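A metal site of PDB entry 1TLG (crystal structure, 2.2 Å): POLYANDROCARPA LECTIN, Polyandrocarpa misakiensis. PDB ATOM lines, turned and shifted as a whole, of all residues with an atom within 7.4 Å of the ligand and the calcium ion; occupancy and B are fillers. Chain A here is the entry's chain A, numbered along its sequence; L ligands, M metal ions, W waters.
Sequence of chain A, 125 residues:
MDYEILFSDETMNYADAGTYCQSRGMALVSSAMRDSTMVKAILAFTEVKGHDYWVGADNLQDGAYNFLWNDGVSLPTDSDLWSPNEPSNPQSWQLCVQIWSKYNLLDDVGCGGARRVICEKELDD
The side-chain hydroxyl of Ser 88 lies close to an oxygen (O3) of the ligand, 3.1 Å away.
The side-chain carboxylate (OE2) of Glu 86 sits close to the side-chain hydroxyl (OG) of Ser 88, 3.3 Å away.
OD2 of Asp 108 sits at hydrogen-bond distance from N of Ser 88 (3.4 Å).
O of Gln 98 sits at hydrogen-bond distance from N of Asp 107.
The side-chain hydroxyl (OH) of Tyr 65 is in hydrogen-bond range of the backbone carbonyl oxygen (O) of Asn 89 (2.5 Å).
The backbone carbonyl oxygen of Ser 88 sits close to the side-chain hydroxyl of Tyr 65 (3.4 Å).
N of Val 109 lies within hydrogen-bond range of O of Cys 96.
The side-chain amide oxygen (OE1) of Gln 98 sits at hydrogen-bond distance from the guanidinium group (NE) of Arg 115 (2.4 Å).
The side-chain carboxylate (OD2) of Asp 52 lies close to the side-chain amide oxygen (OE1) of Gln 98 (3.4 Å).
NE2 of Gln 98 touches C6 of the ligand, at 3.9 Å.
NE1 of Trp 100 touches O6 of the ligand, 3.6 Å away.
CG1 of Val 109 touches O4 of the ligand, at 3.8 Å.
Hydrophobic or aromatic side chains within 4 Å of the ligand: Trp 100 and Val 109.
Within 4 Å of the ligand: Glu 86, Ser 88, Asn 89, Gln 98, Trp 100, Asp 107, Asp 108 and Val 109.
The nearest printed residue that does not touch the ligand is Arg 115 (4.9 Å).
Merely in contact with the calcium ion: Ser 88 (3.7 Å).
Of the 22 residues printed, 5 come within 4 Å of the calcium ion.
Along chain A the residues within 4 Å of the calcium ion span positions 86 to 108.
The nearest printed residue that does not touch the calcium ion is Val 109 (4.7 Å).
The calcium ion is bound by OE1 of Glu 86, OD1 of Asp 108, OD1 of Asp 107, OD1 of Asn 89, O3 of the ligand, O4 of the ligand and O of Asp 108.
Water W3 bridges an oxygen (O2) of the ligand (2.7 Å) and the side-chain hydroxyl (OG) of Ser 88 (2.7 Å).
Water W1 lies within hydrogen-bond range of O6 of the ligand (2.8 Å), NH2 of Arg 115 (2.9 Å), OD2 of Asp 52 (2.9 Å) and NE2 of Gln 98 (3.0 Å).
Water W2 lies within hydrogen-bond range of the side-chain amide nitrogen (ND2) of Asn 89 (2.9 Å) and an oxygen (O5) of the ligand (3.0 Å).
Water W4 bridges an oxygen (O1) of the ligand (2.8 Å) and the side-chain amide nitrogen (ND2) of Asn 89 (3.2 Å).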
ATOM      1  N   ASP A  52      14.734 -35.231  -5.568  1.00  0.00           N
ATOM      2  CA  ASP A  52      14.476 -34.492  -6.796  1.00  0.00           C
ATOM      3  C   ASP A  52      14.104 -35.464  -7.912  1.00  0.00           C
ATOM      4  O   ASP A  52      14.705 -36.529  -8.042  1.00  0.00           O
ATOM      5  CB  ASP A  52      15.717 -33.727  -7.273  1.00  0.00           C
ATOM      6  CG  ASP A  52      16.187 -32.675  -6.303  1.00  0.00           C
ATOM      7  OD1 ASP A  52      15.449 -32.333  -5.352  1.00  0.00           O
ATOM      8  OD2 ASP A  52      17.337 -32.185  -6.462  1.00  0.00           O
ATOM      9  N   TYR A  65      12.142 -17.908 -20.263  1.00  0.00           N
ATOM     10  CA  TYR A  65      11.080 -18.486 -19.441  1.00  0.00           C
ATOM     11  C   TYR A  65       9.871 -18.819 -20.298  1.00  0.00           C
ATOM     12  O   TYR A  65       8.730 -18.633 -19.880  1.00  0.00           O
ATOM     13  CB  TYR A  65      10.720 -17.649 -18.220  1.00  0.00           C
ATOM     14  CG  TYR A  65      11.816 -17.481 -17.187  1.00  0.00           C
ATOM     15  CD1 TYR A  65      12.948 -18.262 -17.130  1.00  0.00           C
ATOM     16  CD2 TYR A  65      11.662 -16.489 -16.210  1.00  0.00           C
ATOM     17  CE1 TYR A  65      13.921 -18.063 -16.161  1.00  0.00           C
ATOM     18  CE2 TYR A  65      12.625 -16.290 -15.245  1.00  0.00           C
ATOM     19  CZ  TYR A  65      13.747 -17.073 -15.217  1.00  0.00           C
ATOM     20  OH  TYR A  65      14.696 -16.857 -14.240  1.00  0.00           O
ATOM     21  N   TRP A  82       4.909 -24.054  -9.534  1.00  0.00           N
ATOM     22  CA  TRP A  82       6.243 -23.621  -9.254  1.00  0.00           C
ATOM     23  C   TRP A  82       6.530 -23.440  -7.759  1.00  0.00           C
ATOM     24  O   TRP A  82       5.739 -22.893  -6.995  1.00  0.00           O
ATOM     25  CB  TRP A  82       6.612 -22.306  -9.971  1.00  0.00           C
ATOM     26  CG  TRP A  82       6.763 -22.322 -11.457  1.00  0.00           C
ATOM     27  CD1 TRP A  82       5.847 -21.860 -12.359  1.00  0.00           C
ATOM     28  CD2 TRP A  82       7.869 -22.801 -12.243  1.00  0.00           C
ATOM     29  NE1 TRP A  82       6.299 -22.030 -13.646  1.00  0.00           N
ATOM     30  CE2 TRP A  82       7.543 -22.606 -13.602  1.00  0.00           C
ATOM     31  CE3 TRP A  82       9.091 -23.393 -11.937  1.00  0.00           C
ATOM     32  CZ2 TRP A  82       8.401 -22.972 -14.637  1.00  0.00           C
ATOM     33  CZ3 TRP A  82       9.936 -23.761 -12.967  1.00  0.00           C
ATOM     34  CH2 TRP A  82       9.599 -23.535 -14.297  1.00  0.00           C
ATOM     35  N   PRO A  84       8.241 -21.668  -4.585  1.00  0.00           N
ATOM     36  CA  PRO A  84       8.331 -20.256  -4.255  1.00  0.00           C
ATOM     37  C   PRO A  84       9.574 -19.643  -4.882  1.00  0.00           C
ATOM     38  O   PRO A  84      10.670 -20.205  -4.792  1.00  0.00           O
ATOM     39  CB  PRO A  84       8.409 -20.218  -2.743  1.00  0.00           C
ATOM     40  CG  PRO A  84       7.867 -21.535  -2.287  1.00  0.00           C
ATOM     41  CD  PRO A  84       8.217 -22.514  -3.370  1.00  0.00           C
ATOM     42  N   ASN A  85       9.401 -18.483  -5.511  1.00  0.00           N
ATOM     43  CA  ASN A  85      10.500 -17.751  -6.119  1.00  0.00           C
ATOM     44  C   ASN A  85      11.178 -18.490  -7.258  1.00  0.00           C
ATOM     45  O   ASN A  85      12.394 -18.331  -7.455  1.00  0.00           O
ATOM     46  CB  ASN A  85      11.555 -17.370  -5.069  1.00  0.00           C
ATOM     47  CG  ASN A  85      11.046 -16.520  -3.931  1.00  0.00           C
ATOM     48  OD1 ASN A  85      11.324 -16.764  -2.749  1.00  0.00           O
ATOM     49  ND2 ASN A  85      10.278 -15.472  -4.236  1.00  0.00           N
ATOM     50  N   GLU A  86      10.422 -19.276  -8.031  1.00  0.00           N
ATOM     51  CA  GLU A  86      10.995 -19.972  -9.200  1.00  0.00           C
ATOM     52  C   GLU A  86       9.935 -19.792 -10.282  1.00  0.00           C
ATOM     53  O   GLU A  86       8.763 -19.632  -9.921  1.00  0.00           O
ATOM     54  CB  GLU A  86      11.281 -21.420  -8.849  1.00  0.00           C
ATOM     55  CG  GLU A  86      12.216 -21.661  -7.682  1.00  0.00           C
ATOM     56  CD  GLU A  86      13.663 -21.301  -7.970  1.00  0.00           C
ATOM     57  OE1 GLU A  86      14.107 -21.269  -9.138  1.00  0.00           O
ATOM     58  OE2 GLU A  86      14.393 -21.056  -6.985  1.00  0.00           O
ATOM     59  N   PRO A  87      10.276 -19.810 -11.548  1.00  0.00           N
ATOM     60  CA  PRO A  87      11.644 -19.991 -12.016  1.00  0.00           C
ATOM     61  C   PRO A  87      12.507 -18.764 -11.767  1.00  0.00           C
ATOM     62  O   PRO A  87      11.985 -17.648 -11.768  1.00  0.00           O
ATOM     63  CB  PRO A  87      11.462 -20.225 -13.509  1.00  0.00           C
ATOM     64  CG  PRO A  87      10.234 -19.470 -13.860  1.00  0.00           C
ATOM     65  CD  PRO A  87       9.323 -19.626 -12.676  1.00  0.00           C
ATOM     66  N   SER A  88      13.801 -18.976 -11.564  1.00  0.00           N
ATOM     67  CA  SER A  88      14.689 -17.873 -11.259  1.00  0.00           C
ATOM     68  C   SER A  88      16.077 -18.011 -11.876  1.00  0.00           C
ATOM     69  O   SER A  88      16.862 -17.082 -11.681  1.00  0.00           O
ATOM     70  CB  SER A  88      14.836 -17.793  -9.724  1.00  0.00           C
ATOM     71  OG  SER A  88      15.570 -18.938  -9.297  1.00  0.00           O
ATOM     72  N   ASN A  89      16.396 -19.109 -12.555  1.00  0.00           N
ATOM     73  CA  ASN A  89      17.746 -19.251 -13.109  1.00  0.00           C
ATOM     74  C   ASN A  89      17.930 -18.276 -14.252  1.00  0.00           C
ATOM     75  O   ASN A  89      16.946 -17.793 -14.830  1.00  0.00           O
ATOM     76  CB  ASN A  89      17.992 -20.700 -13.549  1.00  0.00           C
ATOM     77  CG  ASN A  89      18.159 -21.659 -12.386  1.00  0.00           C
ATOM     78  OD1 ASN A  89      17.445 -21.513 -11.383  1.00  0.00           O
ATOM     79  ND2 ASN A  89      19.090 -22.609 -12.514  1.00  0.00           N
ATOM     80  N   PRO A  90      19.170 -17.993 -14.623  1.00  0.00           N
ATOM     81  CA  PRO A  90      19.453 -17.077 -15.724  1.00  0.00           C
ATOM     82  C   PRO A  90      18.760 -17.527 -17.001  1.00  0.00           C
ATOM     83  O   PRO A  90      18.856 -18.647 -17.486  1.00  0.00           O
ATOM     84  CB  PRO A  90      20.971 -17.076 -15.804  1.00  0.00           C
ATOM     85  CG  PRO A  90      21.429 -17.531 -14.452  1.00  0.00           C
ATOM     86  CD  PRO A  90      20.405 -18.530 -14.003  1.00  0.00           C
ATOM     87  N   TRP A  93      20.322 -19.521 -20.018  1.00  0.00           N
ATOM     88  CA  TRP A  93      20.608 -20.946 -19.924  1.00  0.00           C
ATOM     89  C   TRP A  93      19.545 -21.825 -20.566  1.00  0.00           C
ATOM     90  O   TRP A  93      18.381 -21.469 -20.752  1.00  0.00           O
ATOM     91  CB  TRP A  93      20.672 -21.371 -18.454  1.00  0.00           C
ATOM     92  CG  TRP A  93      21.747 -20.828 -17.565  1.00  0.00           C
ATOM     93  CD1 TRP A  93      22.595 -19.781 -17.795  1.00  0.00           C
ATOM     94  CD2 TRP A  93      22.052 -21.299 -16.238  1.00  0.00           C
ATOM     95  NE1 TRP A  93      23.411 -19.592 -16.713  1.00  0.00           N
ATOM     96  CE2 TRP A  93      23.105 -20.511 -15.739  1.00  0.00           C
ATOM     97  CE3 TRP A  93      21.538 -22.320 -15.428  1.00  0.00           C
ATOM     98  CZ2 TRP A  93      23.656 -20.703 -14.477  1.00  0.00           C
ATOM     99  CZ3 TRP A  93      22.080 -22.512 -14.170  1.00  0.00           C
ATOM    100  CH2 TRP A  93      23.138 -21.701 -13.706  1.00  0.00           C
ATOM    101  N   LEU A  95      17.171 -24.379 -19.779  1.00  0.00           N
ATOM    102  CA  LEU A  95      16.579 -24.738 -18.499  1.00  0.00           C
ATOM    103  C   LEU A  95      15.539 -25.852 -18.596  1.00  0.00           C
ATOM    104  O   LEU A  95      14.620 -25.814 -19.406  1.00  0.00           O
ATOM    105  CB  LEU A  95      15.944 -23.481 -17.849  1.00  0.00           C
ATOM    106  CG  LEU A  95      16.992 -22.413 -17.488  1.00  0.00           C
ATOM    107  CD1 LEU A  95      16.339 -21.053 -17.304  1.00  0.00           C
ATOM    108  CD2 LEU A  95      17.767 -22.803 -16.239  1.00  0.00           C
ATOM    109  N   CYS A  96      15.708 -26.837 -17.730  1.00  0.00           N
ATOM    110  CA  CYS A  96      14.836 -28.009 -17.639  1.00  0.00           C
ATOM    111  C   CYS A  96      14.109 -27.976 -16.304  1.00  0.00           C
ATOM    112  O   CYS A  96      14.578 -27.312 -15.377  1.00  0.00           O
ATOM    113  CB  CYS A  96      15.677 -29.295 -17.772  1.00  0.00           C
ATOM    114  SG  CYS A  96      16.400 -29.423 -19.422  1.00  0.00           S
ATOM    115  N   GLN A  98      12.227 -29.698 -12.879  1.00  0.00           N
ATOM    116  CA  GLN A  98      12.197 -30.803 -11.937  1.00  0.00           C
ATOM    117  C   GLN A  98      11.224 -30.538 -10.793  1.00  0.00           C
ATOM    118  O   GLN A  98      10.809 -29.408 -10.581  1.00  0.00           O
ATOM    119  CB  GLN A  98      13.586 -30.967 -11.282  1.00  0.00           C
ATOM    120  CG  GLN A  98      13.919 -29.794 -10.361  1.00  0.00           C
ATOM    121  CD  GLN A  98      15.038 -29.981  -9.370  1.00  0.00           C
ATOM    122  OE1 GLN A  98      15.500 -31.078  -9.065  1.00  0.00           O
ATOM    123  NE2 GLN A  98      15.552 -28.917  -8.769  1.00  0.00           N
ATOM    124  N   TRP A 100      11.519 -30.248  -7.166  1.00  0.00           N
ATOM    125  CA  TRP A 100      12.594 -29.995  -6.202  1.00  0.00           C
ATOM    126  C   TRP A 100      12.191 -30.375  -4.778  1.00  0.00           C
ATOM    127  O   TRP A 100      11.208 -29.868  -4.262  1.00  0.00           O
ATOM    128  CB  TRP A 100      12.951 -28.521  -6.298  1.00  0.00           C
ATOM    129  CG  TRP A 100      14.125 -28.055  -5.498  1.00  0.00           C
ATOM    130  CD1 TRP A 100      15.159 -28.787  -5.016  1.00  0.00           C
ATOM    131  CD2 TRP A 100      14.403 -26.691  -5.129  1.00  0.00           C
ATOM    132  NE1 TRP A 100      16.060 -27.982  -4.357  1.00  0.00           N
ATOM    133  CE2 TRP A 100      15.614 -26.689  -4.419  1.00  0.00           C
ATOM    134  CE3 TRP A 100      13.739 -25.479  -5.327  1.00  0.00           C
ATOM    135  CZ2 TRP A 100      16.168 -25.520  -3.900  1.00  0.00           C
ATOM    136  CZ3 TRP A 100      14.307 -24.325  -4.819  1.00  0.00           C
ATOM    137  CH2 TRP A 100      15.517 -24.346  -4.107  1.00  0.00           C
ATOM    138  N   LYS A 102      13.264 -29.523  -2.101  1.00  0.00           N
ATOM    139  CA  LYS A 102      13.202 -28.427  -1.126  1.00  0.00           C
ATOM    140  C   LYS A 102      11.744 -28.066  -0.813  1.00  0.00           C
ATOM    141  O   LYS A 102      11.388 -27.787   0.337  1.00  0.00           O
ATOM    142  CB  LYS A 102      13.955 -27.176  -1.550  1.00  0.00           C
ATOM    143  CG  LYS A 102      13.932 -26.123  -0.436  1.00  0.00           C
ATOM    144  CD  LYS A 102      14.834 -24.943  -0.730  1.00  0.00           C
ATOM    145  CE  LYS A 102      14.555 -23.825   0.274  1.00  0.00           C
ATOM    146  NZ  LYS A 102      15.705 -22.880   0.402  1.00  0.00           N
ATOM    147  N   LEU A 106       7.696 -27.505  -8.512  1.00  0.00           N
ATOM    148  CA  LEU A 106       8.507 -27.352  -9.717  1.00  0.00           C
ATOM    149  C   LEU A 106       9.616 -26.318  -9.585  1.00  0.00           C
ATOM    150  O   LEU A 106       9.479 -25.336  -8.859  1.00  0.00           O
ATOM    151  CB  LEU A 106       7.655 -27.029 -10.944  1.00  0.00           C
ATOM    152  CG  LEU A 106       6.608 -28.068 -11.329  1.00  0.00           C
ATOM    153  CD1 LEU A 106       5.944 -27.648 -12.634  1.00  0.00           C
ATOM    154  CD2 LEU A 106       7.184 -29.471 -11.436  1.00  0.00           C
ATOM    155  N   ASP A 107      10.693 -26.550 -10.325  1.00  0.00           N
ATOM    156  CA  ASP A 107      11.840 -25.645 -10.271  1.00  0.00           C
ATOM    157  C   ASP A 107      12.629 -25.703 -11.577  1.00  0.00           C
ATOM    158  O   ASP A 107      12.627 -26.759 -12.185  1.00  0.00           O
ATOM    159  CB  ASP A 107      12.732 -26.019  -9.069  1.00  0.00           C
ATOM    160  CG  ASP A 107      14.081 -25.308  -9.105  1.00  0.00           C
ATOM    161  OD1 ASP A 107      14.071 -24.055  -9.178  1.00  0.00           O
ATOM    162  OD2 ASP A 107      15.141 -25.972  -9.070  1.00  0.00           O
ATOM    163  N   ASP A 108      13.285 -24.610 -11.965  1.00  0.00           N
ATOM    164  CA  ASP A 108      14.104 -24.612 -13.180  1.00  0.00           C
ATOM    165  C   ASP A 108      15.575 -24.836 -12.858  1.00  0.00           C
ATOM    166  O   ASP A 108      16.117 -24.190 -11.953  1.00  0.00           O
ATOM    167  CB  ASP A 108      13.917 -23.302 -13.942  1.00  0.00           C
ATOM    168  CG  ASP A 108      14.370 -22.069 -13.200  1.00  0.00           C
ATOM    169  OD1 ASP A 108      14.233 -21.946 -11.968  1.00  0.00           O
ATOM    170  OD2 ASP A 108      14.901 -21.144 -13.879  1.00  0.00           O
ATOM    171  N   VAL A 109      16.246 -25.716 -13.580  1.00  0.00           N
ATOM    172  CA  VAL A 109      17.640 -26.056 -13.347  1.00  0.00           C
ATOM    173  C   VAL A 109      18.398 -26.278 -14.648  1.00  0.00           C
ATOM    174  O   VAL A 109      17.799 -26.345 -15.717  1.00  0.00           O
ATOM    175  CB  VAL A 109      17.744 -27.400 -12.599  1.00  0.00           C
ATOM    176  CG1 VAL A 109      17.255 -27.280 -11.173  1.00  0.00           C
ATOM    177  CG2 VAL A 109      16.944 -28.463 -13.346  1.00  0.00           C
ATOM    178  N   GLY A 110      19.712 -26.463 -14.518  1.00  0.00           N
ATOM    179  CA  GLY A 110      20.521 -26.807 -15.693  1.00  0.00           C
ATOM    180  C   GLY A 110      20.093 -28.259 -16.000  1.00  0.00           C
ATOM    181  O   GLY A 110      19.540 -28.929 -15.108  1.00  0.00           O
ATOM    182  N   ARG A 115      19.006 -36.945 -11.711  1.00  0.00           N
ATOM    183  CA  ARG A 115      17.825 -36.944 -10.850  1.00  0.00           C
ATOM    184  C   ARG A 115      16.944 -38.144 -11.211  1.00  0.00           C
ATOM    185  O   ARG A 115      17.112 -38.751 -12.256  1.00  0.00           O
ATOM    186  CB  ARG A 115      17.012 -35.667 -10.996  1.00  0.00           C
ATOM    187  CG  ARG A 115      17.789 -34.373 -10.817  1.00  0.00           C
ATOM    188  CD  ARG A 115      16.857 -33.171 -10.998  1.00  0.00           C
ATOM    189  NE  ARG A 115      17.418 -32.047 -10.215  1.00  0.00           N
ATOM    190  CZ  ARG A 115      18.455 -31.339 -10.676  1.00  0.00           C
ATOM    191  NH1 ARG A 115      18.982 -31.587 -11.867  1.00  0.00           N
ATOM    192  NH2 ARG A 115      18.953 -30.354  -9.939  1.00  0.00           N
HETATM  193  C1  LIG L   1      19.777 -23.081  -7.021  1.00  0.00           C
HETATM  194  C2  LIG L   1      18.825 -22.105  -7.699  1.00  0.00           C
HETATM  195  C3  LIG L   1      17.398 -22.461  -7.356  1.00  0.00           C
HETATM  196  C4  LIG L   1      17.062 -23.958  -7.628  1.00  0.00           C
HETATM  197  C5  LIG L   1      18.123 -24.852  -6.941  1.00  0.00           C
HETATM  198  C6  LIG L   1      17.978 -26.373  -7.151  1.00  0.00           C
HETATM  199  O1  LIG L   1      21.072 -22.826  -7.449  1.00  0.00           O
HETATM  200  O2  LIG L   1      19.078 -20.789  -7.197  1.00  0.00           O
HETATM  201  O3  LIG L   1      16.585 -21.652  -8.128  1.00  0.00           O
HETATM  202  O4  LIG L   1      16.974 -24.129  -8.999  1.00  0.00           O
HETATM  203  O5  LIG L   1      19.455 -24.437  -7.361  1.00  0.00           O
HETATM  204  O6  LIG L   1      18.930 -27.058  -6.363  1.00  0.00           O
HETATM  205 CA    CA M   1      15.551 -22.483 -10.193  1.00  0.00          CA
HETATM  206  O   HOH W   1      18.152 -29.521  -7.319  1.00  0.00           O
HETATM  207  O   HOH W   2      19.423 -24.434 -10.337  1.00  0.00           O
HETATM  208  O   HOH W   3      18.303 -19.193  -9.225  1.00  0.00           O
HETATM  209  O   HOH W   4      21.190 -22.116 -10.185  1.00  0.00           O
HETATM  210  O   HOH W   5      21.960 -20.139  -7.411  1.00  0.00           O
